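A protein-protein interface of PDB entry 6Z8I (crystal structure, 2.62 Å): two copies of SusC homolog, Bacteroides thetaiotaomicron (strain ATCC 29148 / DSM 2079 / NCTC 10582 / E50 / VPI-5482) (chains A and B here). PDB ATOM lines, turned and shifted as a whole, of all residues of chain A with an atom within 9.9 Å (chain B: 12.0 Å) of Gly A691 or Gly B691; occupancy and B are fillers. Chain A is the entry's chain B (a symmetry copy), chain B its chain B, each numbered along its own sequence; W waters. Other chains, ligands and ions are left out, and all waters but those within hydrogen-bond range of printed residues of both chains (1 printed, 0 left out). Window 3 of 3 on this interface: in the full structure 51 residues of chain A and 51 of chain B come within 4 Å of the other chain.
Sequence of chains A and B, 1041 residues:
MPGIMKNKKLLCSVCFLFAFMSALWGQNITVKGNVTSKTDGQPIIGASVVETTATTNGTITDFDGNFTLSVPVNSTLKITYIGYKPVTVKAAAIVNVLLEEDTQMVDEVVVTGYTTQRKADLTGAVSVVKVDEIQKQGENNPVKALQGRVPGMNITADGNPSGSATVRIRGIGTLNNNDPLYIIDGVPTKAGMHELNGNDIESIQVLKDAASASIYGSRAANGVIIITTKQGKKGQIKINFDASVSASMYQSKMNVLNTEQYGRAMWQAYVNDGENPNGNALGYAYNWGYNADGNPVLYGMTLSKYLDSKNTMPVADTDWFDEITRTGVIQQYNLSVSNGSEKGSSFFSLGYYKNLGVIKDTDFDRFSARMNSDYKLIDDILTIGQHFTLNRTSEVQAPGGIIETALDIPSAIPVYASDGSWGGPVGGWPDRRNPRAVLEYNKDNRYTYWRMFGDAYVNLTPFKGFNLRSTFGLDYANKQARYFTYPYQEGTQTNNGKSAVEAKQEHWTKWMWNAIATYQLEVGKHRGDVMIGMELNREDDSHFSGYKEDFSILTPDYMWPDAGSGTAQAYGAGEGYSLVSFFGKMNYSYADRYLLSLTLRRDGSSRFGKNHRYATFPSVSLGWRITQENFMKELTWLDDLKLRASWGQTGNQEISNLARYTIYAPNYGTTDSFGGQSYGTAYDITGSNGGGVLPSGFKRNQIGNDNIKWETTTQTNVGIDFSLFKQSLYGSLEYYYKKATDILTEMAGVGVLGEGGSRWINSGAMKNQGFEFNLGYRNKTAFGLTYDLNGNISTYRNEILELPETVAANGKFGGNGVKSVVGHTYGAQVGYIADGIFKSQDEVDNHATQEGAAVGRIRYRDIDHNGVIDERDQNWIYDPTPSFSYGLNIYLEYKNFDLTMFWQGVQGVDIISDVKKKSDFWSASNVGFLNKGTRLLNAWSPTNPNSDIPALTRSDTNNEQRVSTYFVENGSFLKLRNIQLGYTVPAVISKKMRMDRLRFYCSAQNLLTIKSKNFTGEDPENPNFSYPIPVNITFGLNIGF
Water W1 lies within hydrogen-bond range of O of Leu A694 (2.7 Å) and O of Ser B565 (3.4 Å).
Of the 18 printed residues of chain B, 4 touch a printed residue of chain A.
Hydrophobic or aromatic side chains of chain A that line the printed part of chain B: Tyr A668 and Val A693.
Along chain A the printed residues that touch a printed residue of chain B span positions 567 to 693.
Among the printed residues, 5 pairs touch across the chains.
Among the printed residues, no Asp or Glu carboxylate lies within 4 Å of a Lys or Arg side-chain nitrogen of the other chain.
Thr A567 touches Val B693, and with the chains exchanged Val A693 touches Thr B567.
Gly B691 touches its own counterpart, Gly A691.
13 positions are printed for both chains.
Of the 5 pairs that touch across the chains among the printed residues, 3 have their exchanged pair printed and touching as well.
Of the printed residues of chain B, Tyr A668 touches Ser B565 (3.2 Å).
No residue of chain B comes within 4 Å of Asn A689.
Gly A690 touches none of the printed residues of chain B.
Printed residues of chain B within 4 Å of Gly A691: Gly B691.
No residue of chain B comes within 4 Å of Gly A692.
Of the printed residues of chain B, Val A693 touches Ser B565 and Thr B567.
No residue of chain A comes within 4 Å of Gly B690.
Gly B691 touches one residue of chain A.
Gly B692 touches none of the printed residues of chain A.
The nearest residue of chain B that does not touch Gly A691 is Gly B692 (4.9 Å).
The nearest residue of chain A that does not touch Gly B691 is Gly A692 (4.9 Å).
The side-chain hydroxyl (OH) of Tyr A668 sits at hydrogen-bond distance from the backbone NH (N) of Leu A694, 2.9 Å away.
Val B693 touches Thr A567 (CG2 to CG2, 3.6 Å).
CE2 of Tyr A668 touches O of Ser B565, at 3.2 Å.
Gly B691 touches Gly A691.
Val A693 touches Ser B565.
CG2 of Thr B567 touches CG2 of Val A693 (3.6 Å).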
ATOM      1  N   THR A 567     -15.497  23.378   7.041  1.00  0.00           N
ATOM      2  CA  THR A 567     -16.851  23.620   6.562  1.00  0.00           C
ATOM      3  C   THR A 567     -17.426  24.896   7.166  1.00  0.00           C
ATOM      4  O   THR A 567     -16.944  25.429   8.173  1.00  0.00           O
ATOM      5  CB  THR A 567     -17.793  22.463   6.906  1.00  0.00           C
ATOM      6  OG1 THR A 567     -17.595  22.083   8.271  1.00  0.00           O
ATOM      7  CG2 THR A 567     -17.552  21.261   5.987  1.00  0.00           C
ATOM      8  N   TYR A 668     -32.646  21.940   8.954  1.00  0.00           N
ATOM      9  CA  TYR A 668     -31.845  20.860   8.381  1.00  0.00           C
ATOM     10  C   TYR A 668     -30.948  20.222   9.432  1.00  0.00           C
ATOM     11  O   TYR A 668     -30.788  18.990   9.455  1.00  0.00           O
ATOM     12  CB  TYR A 668     -31.027  21.417   7.219  1.00  0.00           C
ATOM     13  CG  TYR A 668     -30.101  20.482   6.443  1.00  0.00           C
ATOM     14  CD1 TYR A 668     -28.847  20.108   6.953  1.00  0.00           C
ATOM     15  CD2 TYR A 668     -30.432  20.061   5.155  1.00  0.00           C
ATOM     16  CE1 TYR A 668     -27.975  19.302   6.222  1.00  0.00           C
ATOM     17  CE2 TYR A 668     -29.568  19.257   4.412  1.00  0.00           C
ATOM     18  CZ  TYR A 668     -28.338  18.882   4.946  1.00  0.00           C
ATOM     19  OH  TYR A 668     -27.487  18.077   4.197  1.00  0.00           O
ATOM     20  N   ASP A 684     -30.089  10.702   5.434  1.00  0.00           N
ATOM     21  CA  ASP A 684     -29.436   9.903   4.406  1.00  0.00           C
ATOM     22  C   ASP A 684     -30.350   8.831   3.819  1.00  0.00           C
ATOM     23  O   ASP A 684     -30.060   7.628   3.919  1.00  0.00           O
ATOM     24  CB  ASP A 684     -28.185   9.255   4.999  1.00  0.00           C
ATOM     25  CG  ASP A 684     -27.349   8.564   3.965  1.00  0.00           C
ATOM     26  OD1 ASP A 684     -26.604   7.635   4.358  1.00  0.00           O
ATOM     27  OD2 ASP A 684     -27.452   8.947   2.769  1.00  0.00           O
ATOM     28  N   THR A 686     -30.818   7.589   1.058  1.00  0.00           N
ATOM     29  CA  THR A 686     -30.259   6.692   0.048  1.00  0.00           C
ATOM     30  C   THR A 686     -29.216   5.717   0.590  1.00  0.00           C
ATOM     31  O   THR A 686     -28.932   4.716  -0.074  1.00  0.00           O
ATOM     32  CB  THR A 686     -29.614   7.478  -1.100  1.00  0.00           C
ATOM     33  OG1 THR A 686     -28.478   8.192  -0.612  1.00  0.00           O
ATOM     34  CG2 THR A 686     -30.602   8.446  -1.724  1.00  0.00           C
ATOM     35  N   GLY A 687     -28.658   5.952   1.780  1.00  0.00           N
ATOM     36  CA  GLY A 687     -27.656   5.058   2.329  1.00  0.00           C
ATOM     37  C   GLY A 687     -26.238   5.388   1.923  1.00  0.00           C
ATOM     38  O   GLY A 687     -25.310   4.684   2.337  1.00  0.00           O
ATOM     39  N   SER A 688     -26.055   6.424   1.107  1.00  0.00           N
ATOM     40  CA  SER A 688     -24.770   6.994   0.737  1.00  0.00           C
ATOM     41  C   SER A 688     -23.750   6.982   1.868  1.00  0.00           C
ATOM     42  O   SER A 688     -22.586   6.637   1.671  1.00  0.00           O
ATOM     43  CB  SER A 688     -24.991   8.438   0.294  1.00  0.00           C
ATOM     44  OG  SER A 688     -25.291   9.256   1.416  1.00  0.00           O
ATOM     45  N   ASN A 689     -24.175   7.434   3.038  1.00  0.00           N
ATOM     46  CA  ASN A 689     -23.430   7.706   4.277  1.00  0.00           C
ATOM     47  C   ASN A 689     -22.996   9.163   4.281  1.00  0.00           C
ATOM     48  O   ASN A 689     -22.235   9.563   5.182  1.00  0.00           O
ATOM     49  CB  ASN A 689     -22.226   6.787   4.529  1.00  0.00           C
ATOM     50  CG  ASN A 689     -21.918   6.634   6.008  1.00  0.00           C
ATOM     51  OD1 ASN A 689     -22.818   6.326   6.844  1.00  0.00           O
ATOM     52  ND2 ASN A 689     -20.642   6.834   6.356  1.00  0.00           N
ATOM     53  N   GLY A 690     -23.414   9.968   3.302  1.00  0.00           N
ATOM     54  CA  GLY A 690     -23.221  11.406   3.360  1.00  0.00           C
ATOM     55  C   GLY A 690     -22.432  11.930   2.178  1.00  0.00           C
ATOM     56  O   GLY A 690     -22.710  11.558   1.014  1.00  0.00           O
ATOM     57  N   GLY A 691     -21.491  12.817   2.455  1.00  0.00           N
ATOM     58  CA  GLY A 691     -20.721  13.441   1.395  1.00  0.00           C
ATOM     59  C   GLY A 691     -21.541  14.214   0.384  1.00  0.00           C
ATOM     60  O   GLY A 691     -21.265  14.140  -0.821  1.00  0.00           O
ATOM     61  N   GLY A 692     -22.531  14.960   0.840  1.00  0.00           N
ATOM     62  CA  GLY A 692     -23.313  15.785  -0.058  1.00  0.00           C
ATOM     63  C   GLY A 692     -24.439  16.416   0.720  1.00  0.00           C
ATOM     64  O   GLY A 692     -24.582  16.209   1.927  1.00  0.00           O
ATOM     65  N   VAL A 693     -25.227  17.216   0.014  1.00  0.00           N
ATOM     66  CA  VAL A 693     -26.477  17.689   0.583  1.00  0.00           C
ATOM     67  C   VAL A 693     -27.421  16.501   0.747  1.00  0.00           C
ATOM     68  O   VAL A 693     -27.731  15.787  -0.217  1.00  0.00           O
ATOM     69  CB  VAL A 693     -27.096  18.779  -0.293  1.00  0.00           C
ATOM     70  CG1 VAL A 693     -28.451  19.181   0.246  1.00  0.00           C
ATOM     71  CG2 VAL A 693     -26.179  19.970  -0.337  1.00  0.00           C
ATOM     72  N   LEU A 694     -27.870  16.275   1.978  1.00  0.00           N
ATOM     73  CA  LEU A 694     -28.944  15.335   2.237  1.00  0.00           C
ATOM     74  C   LEU A 694     -30.294  15.934   1.838  1.00  0.00           C
ATOM     75  O   LEU A 694     -30.492  17.152   1.918  1.00  0.00           O
ATOM     76  CB  LEU A 694     -28.972  14.965   3.716  1.00  0.00           C
ATOM     77  CG  LEU A 694     -27.713  14.387   4.365  1.00  0.00           C
ATOM     78  CD1 LEU A 694     -27.975  14.119   5.858  1.00  0.00           C
ATOM     79  CD2 LEU A 694     -27.344  13.113   3.664  1.00  0.00           C
ATOM     80  N   PRO A 695     -31.244  15.105   1.410  1.00  0.00           N
ATOM     81  CA  PRO A 695     -32.645  15.557   1.389  1.00  0.00           C
ATOM     82  C   PRO A 695     -33.106  15.878   2.805  1.00  0.00           C
ATOM     83  O   PRO A 695     -32.563  15.368   3.789  1.00  0.00           O
ATOM     84  CB  PRO A 695     -33.400  14.355   0.802  1.00  0.00           C
ATOM     85  CG  PRO A 695     -32.510  13.167   1.082  1.00  0.00           C
ATOM     86  CD  PRO A 695     -31.105  13.689   1.011  1.00  0.00           C
ATOM     87  N   SER B 565     -31.718  24.784   2.790  1.00  0.00           N
ATOM     88  CA  SER B 565     -31.452  23.353   2.918  1.00  0.00           C
ATOM     89  C   SER B 565     -30.202  22.872   2.204  1.00  0.00           C
ATOM     90  O   SER B 565     -29.748  21.766   2.499  1.00  0.00           O
ATOM     91  CB  SER B 565     -32.631  22.533   2.389  1.00  0.00           C
ATOM     92  OG  SER B 565     -33.072  23.046   1.147  1.00  0.00           O
ATOM     93  N   GLY B 566     -29.649  23.649   1.273  1.00  0.00           N
ATOM     94  CA  GLY B 566     -28.409  23.309   0.604  1.00  0.00           C
ATOM     95  C   GLY B 566     -27.188  23.732   1.395  1.00  0.00           C
ATOM     96  O   GLY B 566     -27.243  23.963   2.606  1.00  0.00           O
ATOM     97  N   THR B 567     -26.059  23.818   0.692  1.00  0.00           N
ATOM     98  CA  THR B 567     -24.788  24.100   1.345  1.00  0.00           C
ATOM     99  C   THR B 567     -24.651  25.585   1.662  1.00  0.00           C
ATOM    100  O   THR B 567     -25.354  26.446   1.121  1.00  0.00           O
ATOM    101  CB  THR B 567     -23.596  23.686   0.477  1.00  0.00           C
ATOM    102  OG1 THR B 567     -23.807  24.144  -0.862  1.00  0.00           O
ATOM    103  CG2 THR B 567     -23.404  22.167   0.487  1.00  0.00           C
ATOM    104  N   TYR B 668      -9.447  28.645  -0.090  1.00  0.00           N
ATOM    105  CA  TYR B 668      -9.857  27.265  -0.339  1.00  0.00           C
ATOM    106  C   TYR B 668     -10.634  27.145  -1.642  1.00  0.00           C
ATOM    107  O   TYR B 668     -10.446  26.179  -2.400  1.00  0.00           O
ATOM    108  CB  TYR B 668     -10.686  26.776   0.846  1.00  0.00           C
ATOM    109  CG  TYR B 668     -11.238  25.351   0.835  1.00  0.00           C
ATOM    110  CD1 TYR B 668     -12.379  25.016   0.088  1.00  0.00           C
ATOM    111  CD2 TYR B 668     -10.683  24.368   1.654  1.00  0.00           C
ATOM    112  CE1 TYR B 668     -12.919  23.731   0.121  1.00  0.00           C
ATOM    113  CE2 TYR B 668     -11.215  23.079   1.698  1.00  0.00           C
ATOM    114  CZ  TYR B 668     -12.336  22.764   0.934  1.00  0.00           C
ATOM    115  OH  TYR B 668     -12.854  21.475   0.985  1.00  0.00           O
ATOM    116  N   ALA B 682      -7.637  24.063  -2.392  1.00  0.00           N
ATOM    117  CA  ALA B 682      -8.144  22.755  -2.004  1.00  0.00           C
ATOM    118  C   ALA B 682      -8.009  21.773  -3.160  1.00  0.00           C
ATOM    119  O   ALA B 682      -8.325  22.101  -4.307  1.00  0.00           O
ATOM    120  CB  ALA B 682      -9.606  22.847  -1.590  1.00  0.00           C
ATOM    121  N   TYR B 683      -7.563  20.557  -2.844  1.00  0.00           N
ATOM    122  CA  TYR B 683      -7.420  19.511  -3.839  1.00  0.00           C
ATOM    123  C   TYR B 683      -7.760  18.135  -3.267  1.00  0.00           C
ATOM    124  O   TYR B 683      -7.389  17.799  -2.136  1.00  0.00           O
ATOM    125  CB  TYR B 683      -6.003  19.489  -4.379  1.00  0.00           C
ATOM    126  CG  TYR B 683      -5.807  18.645  -5.624  1.00  0.00           C
ATOM    127  CD1 TYR B 683      -6.387  19.023  -6.830  1.00  0.00           C
ATOM    128  CD2 TYR B 683      -5.034  17.479  -5.593  1.00  0.00           C
ATOM    129  CE1 TYR B 683      -6.206  18.271  -7.964  1.00  0.00           C
ATOM    130  CE2 TYR B 683      -4.843  16.730  -6.726  1.00  0.00           C
ATOM    131  CZ  TYR B 683      -5.421  17.136  -7.915  1.00  0.00           C
ATOM    132  OH  TYR B 683      -5.230  16.427  -9.074  1.00  0.00           O
ATOM    133  N   ASP B 684      -8.421  17.326  -4.098  1.00  0.00           N
ATOM    134  CA  ASP B 684      -8.726  15.934  -3.802  1.00  0.00           C
ATOM    135  C   ASP B 684      -7.497  15.030  -3.874  1.00  0.00           C
ATOM    136  O   ASP B 684      -7.447  14.094  -4.688  1.00  0.00           O
ATOM    137  CB  ASP B 684      -9.794  15.440  -4.777  1.00  0.00           C
ATOM    138  CG  ASP B 684     -10.304  14.074  -4.428  1.00  0.00           C
ATOM    139  OD1 ASP B 684     -10.793  13.391  -5.360  1.00  0.00           O
ATOM    140  OD2 ASP B 684     -10.201  13.691  -3.233  1.00  0.00           O
ATOM    141  N   ILE B 685      -6.510  15.278  -3.008  1.00  0.00           N
ATOM    142  CA  ILE B 685      -5.227  14.591  -3.134  1.00  0.00           C
ATOM    143  C   ILE B 685      -5.359  13.081  -2.975  1.00  0.00           C
ATOM    144  O   ILE B 685      -4.471  12.341  -3.420  1.00  0.00           O
ATOM    145  CB  ILE B 685      -4.221  15.142  -2.102  1.00  0.00           C
ATOM    146  CG1 ILE B 685      -2.780  14.722  -2.445  1.00  0.00           C
ATOM    147  CG2 ILE B 685      -4.605  14.671  -0.696  1.00  0.00           C
ATOM    148  CD1 ILE B 685      -2.266  15.243  -3.822  1.00  0.00           C
ATOM    149  N   THR B 686      -6.445  12.596  -2.340  1.00  0.00           N
ATOM    150  CA  THR B 686      -6.634  11.166  -2.107  1.00  0.00           C
ATOM    151  C   THR B 686      -7.408  10.452  -3.213  1.00  0.00           C
ATOM    152  O   THR B 686      -7.338   9.222  -3.294  1.00  0.00           O
ATOM    153  CB  THR B 686      -7.363  10.908  -0.783  1.00  0.00           C
ATOM    154  OG1 THR B 686      -8.694  11.419  -0.862  1.00  0.00           O
ATOM    155  CG2 THR B 686      -6.632  11.553   0.380  1.00  0.00           C
ATOM    156  N   GLY B 687      -8.119  11.173  -4.083  1.00  0.00           N
ATOM    157  CA  GLY B 687      -8.877  10.536  -5.143  1.00  0.00           C
ATOM    158  C   GLY B 687     -10.287  10.152  -4.756  1.00  0.00           C
ATOM    159  O   GLY B 687     -11.015   9.601  -5.589  1.00  0.00           O
ATOM    160  N   SER B 688     -10.675  10.408  -3.508  1.00  0.00           N
ATOM    161  CA  SER B 688     -12.028  10.265  -2.996  1.00  0.00           C
ATOM    162  C   SER B 688     -13.105  10.635  -4.007  1.00  0.00           C
ATOM    163  O   SER B 688     -14.102   9.931  -4.160  1.00  0.00           O
ATOM    164  CB  SER B 688     -12.179  11.163  -1.771  1.00  0.00           C
ATOM    165  OG  SER B 688     -12.226  12.527  -2.165  1.00  0.00           O
ATOM    166  N   ASN B 689     -12.934  11.784  -4.643  1.00  0.00           N
ATOM    167  CA  ASN B 689     -13.838  12.510  -5.549  1.00  0.00           C
ATOM    168  C   ASN B 689     -14.660  13.498  -4.737  1.00  0.00           C
ATOM    169  O   ASN B 689     -15.583  14.118  -5.298  1.00  0.00           O
ATOM    170  CB  ASN B 689     -14.755  11.623  -6.404  1.00  0.00           C
ATOM    171  CG  ASN B 689     -15.144  12.290  -7.711  1.00  0.00           C
ATOM    172  OD1 ASN B 689     -14.276  12.798  -8.480  1.00  0.00           O
ATOM    173  ND2 ASN B 689     -16.452  12.289  -7.993  1.00  0.00           N
ATOM    174  N   GLY B 690     -14.395  13.651  -3.438  1.00  0.00           N
ATOM    175  CA  GLY B 690     -14.986  14.724  -2.659  1.00  0.00           C
ATOM    176  C   GLY B 690     -15.777  14.207  -1.474  1.00  0.00           C
ATOM    177  O   GLY B 690     -15.298  13.318  -0.731  1.00  0.00           O
ATOM    178  N   GLY B 691     -16.950  14.780  -1.264  1.00  0.00           N
ATOM    179  CA  GLY B 691     -17.761  14.416  -0.117  1.00  0.00           C
ATOM    180  C   GLY B 691     -17.100  14.638   1.226  1.00  0.00           C
ATOM    181  O   GLY B 691     -17.230  13.798   2.126  1.00  0.00           O
ATOM    182  N   GLY B 692     -16.405  15.750   1.390  1.00  0.00           N
ATOM    183  CA  GLY B 692     -15.804  16.068   2.669  1.00  0.00           C
ATOM    184  C   GLY B 692     -14.977  17.319   2.520  1.00  0.00           C
ATOM    185  O   GLY B 692     -14.895  17.910   1.441  1.00  0.00           O
ATOM    186  N   VAL B 693     -14.382  17.732   3.630  1.00  0.00           N
ATOM    187  CA  VAL B 693     -13.373  18.775   3.567  1.00  0.00           C
ATOM    188  C   VAL B 693     -12.154  18.233   2.826  1.00  0.00           C
ATOM    189  O   VAL B 693     -11.568  17.212   3.211  1.00  0.00           O
ATOM    190  CB  VAL B 693     -13.004  19.261   4.970  1.00  0.00           C
ATOM    191  CG1 VAL B 693     -11.873  20.262   4.899  1.00  0.00           C
ATOM    192  CG2 VAL B 693     -14.209  19.884   5.619  1.00  0.00           C
ATOM    193  N   LEU B 694     -11.777  18.910   1.745  1.00  0.00           N
ATOM    194  CA  LEU B 694     -10.511  18.648   1.086  1.00  0.00           C
ATOM    195  C   LEU B 694      -9.352  19.247   1.885  1.00  0.00           C
ATOM    196  O   LEU B 694      -9.510  20.274   2.554  1.00  0.00           O
ATOM    197  CB  LEU B 694     -10.520  19.244  -0.318  1.00  0.00           C
ATOM    198  CG  LEU B 694     -11.622  18.834  -1.297  1.00  0.00           C
ATOM    199  CD1 LEU B 694     -11.435  19.580  -2.630  1.00  0.00           C
ATOM    200  CD2 LEU B 694     -11.552  17.351  -1.516  1.00  0.00           C
ATOM    201  N   PRO B 695      -8.173  18.631   1.830  1.00  0.00           N
ATOM    202  CA  PRO B 695      -6.959  19.354   2.243  1.00  0.00           C
ATOM    203  C   PRO B 695      -6.739  20.558   1.336  1.00  0.00           C
ATOM    204  O   PRO B 695      -7.208  20.597   0.195  1.00  0.00           O
ATOM    205  CB  PRO B 695      -5.846  18.307   2.080  1.00  0.00           C
ATOM    206  CG  PRO B 695      -6.390  17.320   1.074  1.00  0.00           C
ATOM    207  CD  PRO B 695      -7.872  17.282   1.307  1.00  0.00           C
HETATM  208  O   HOH W   1     -31.825  19.376   1.154  1.00  0.00           O
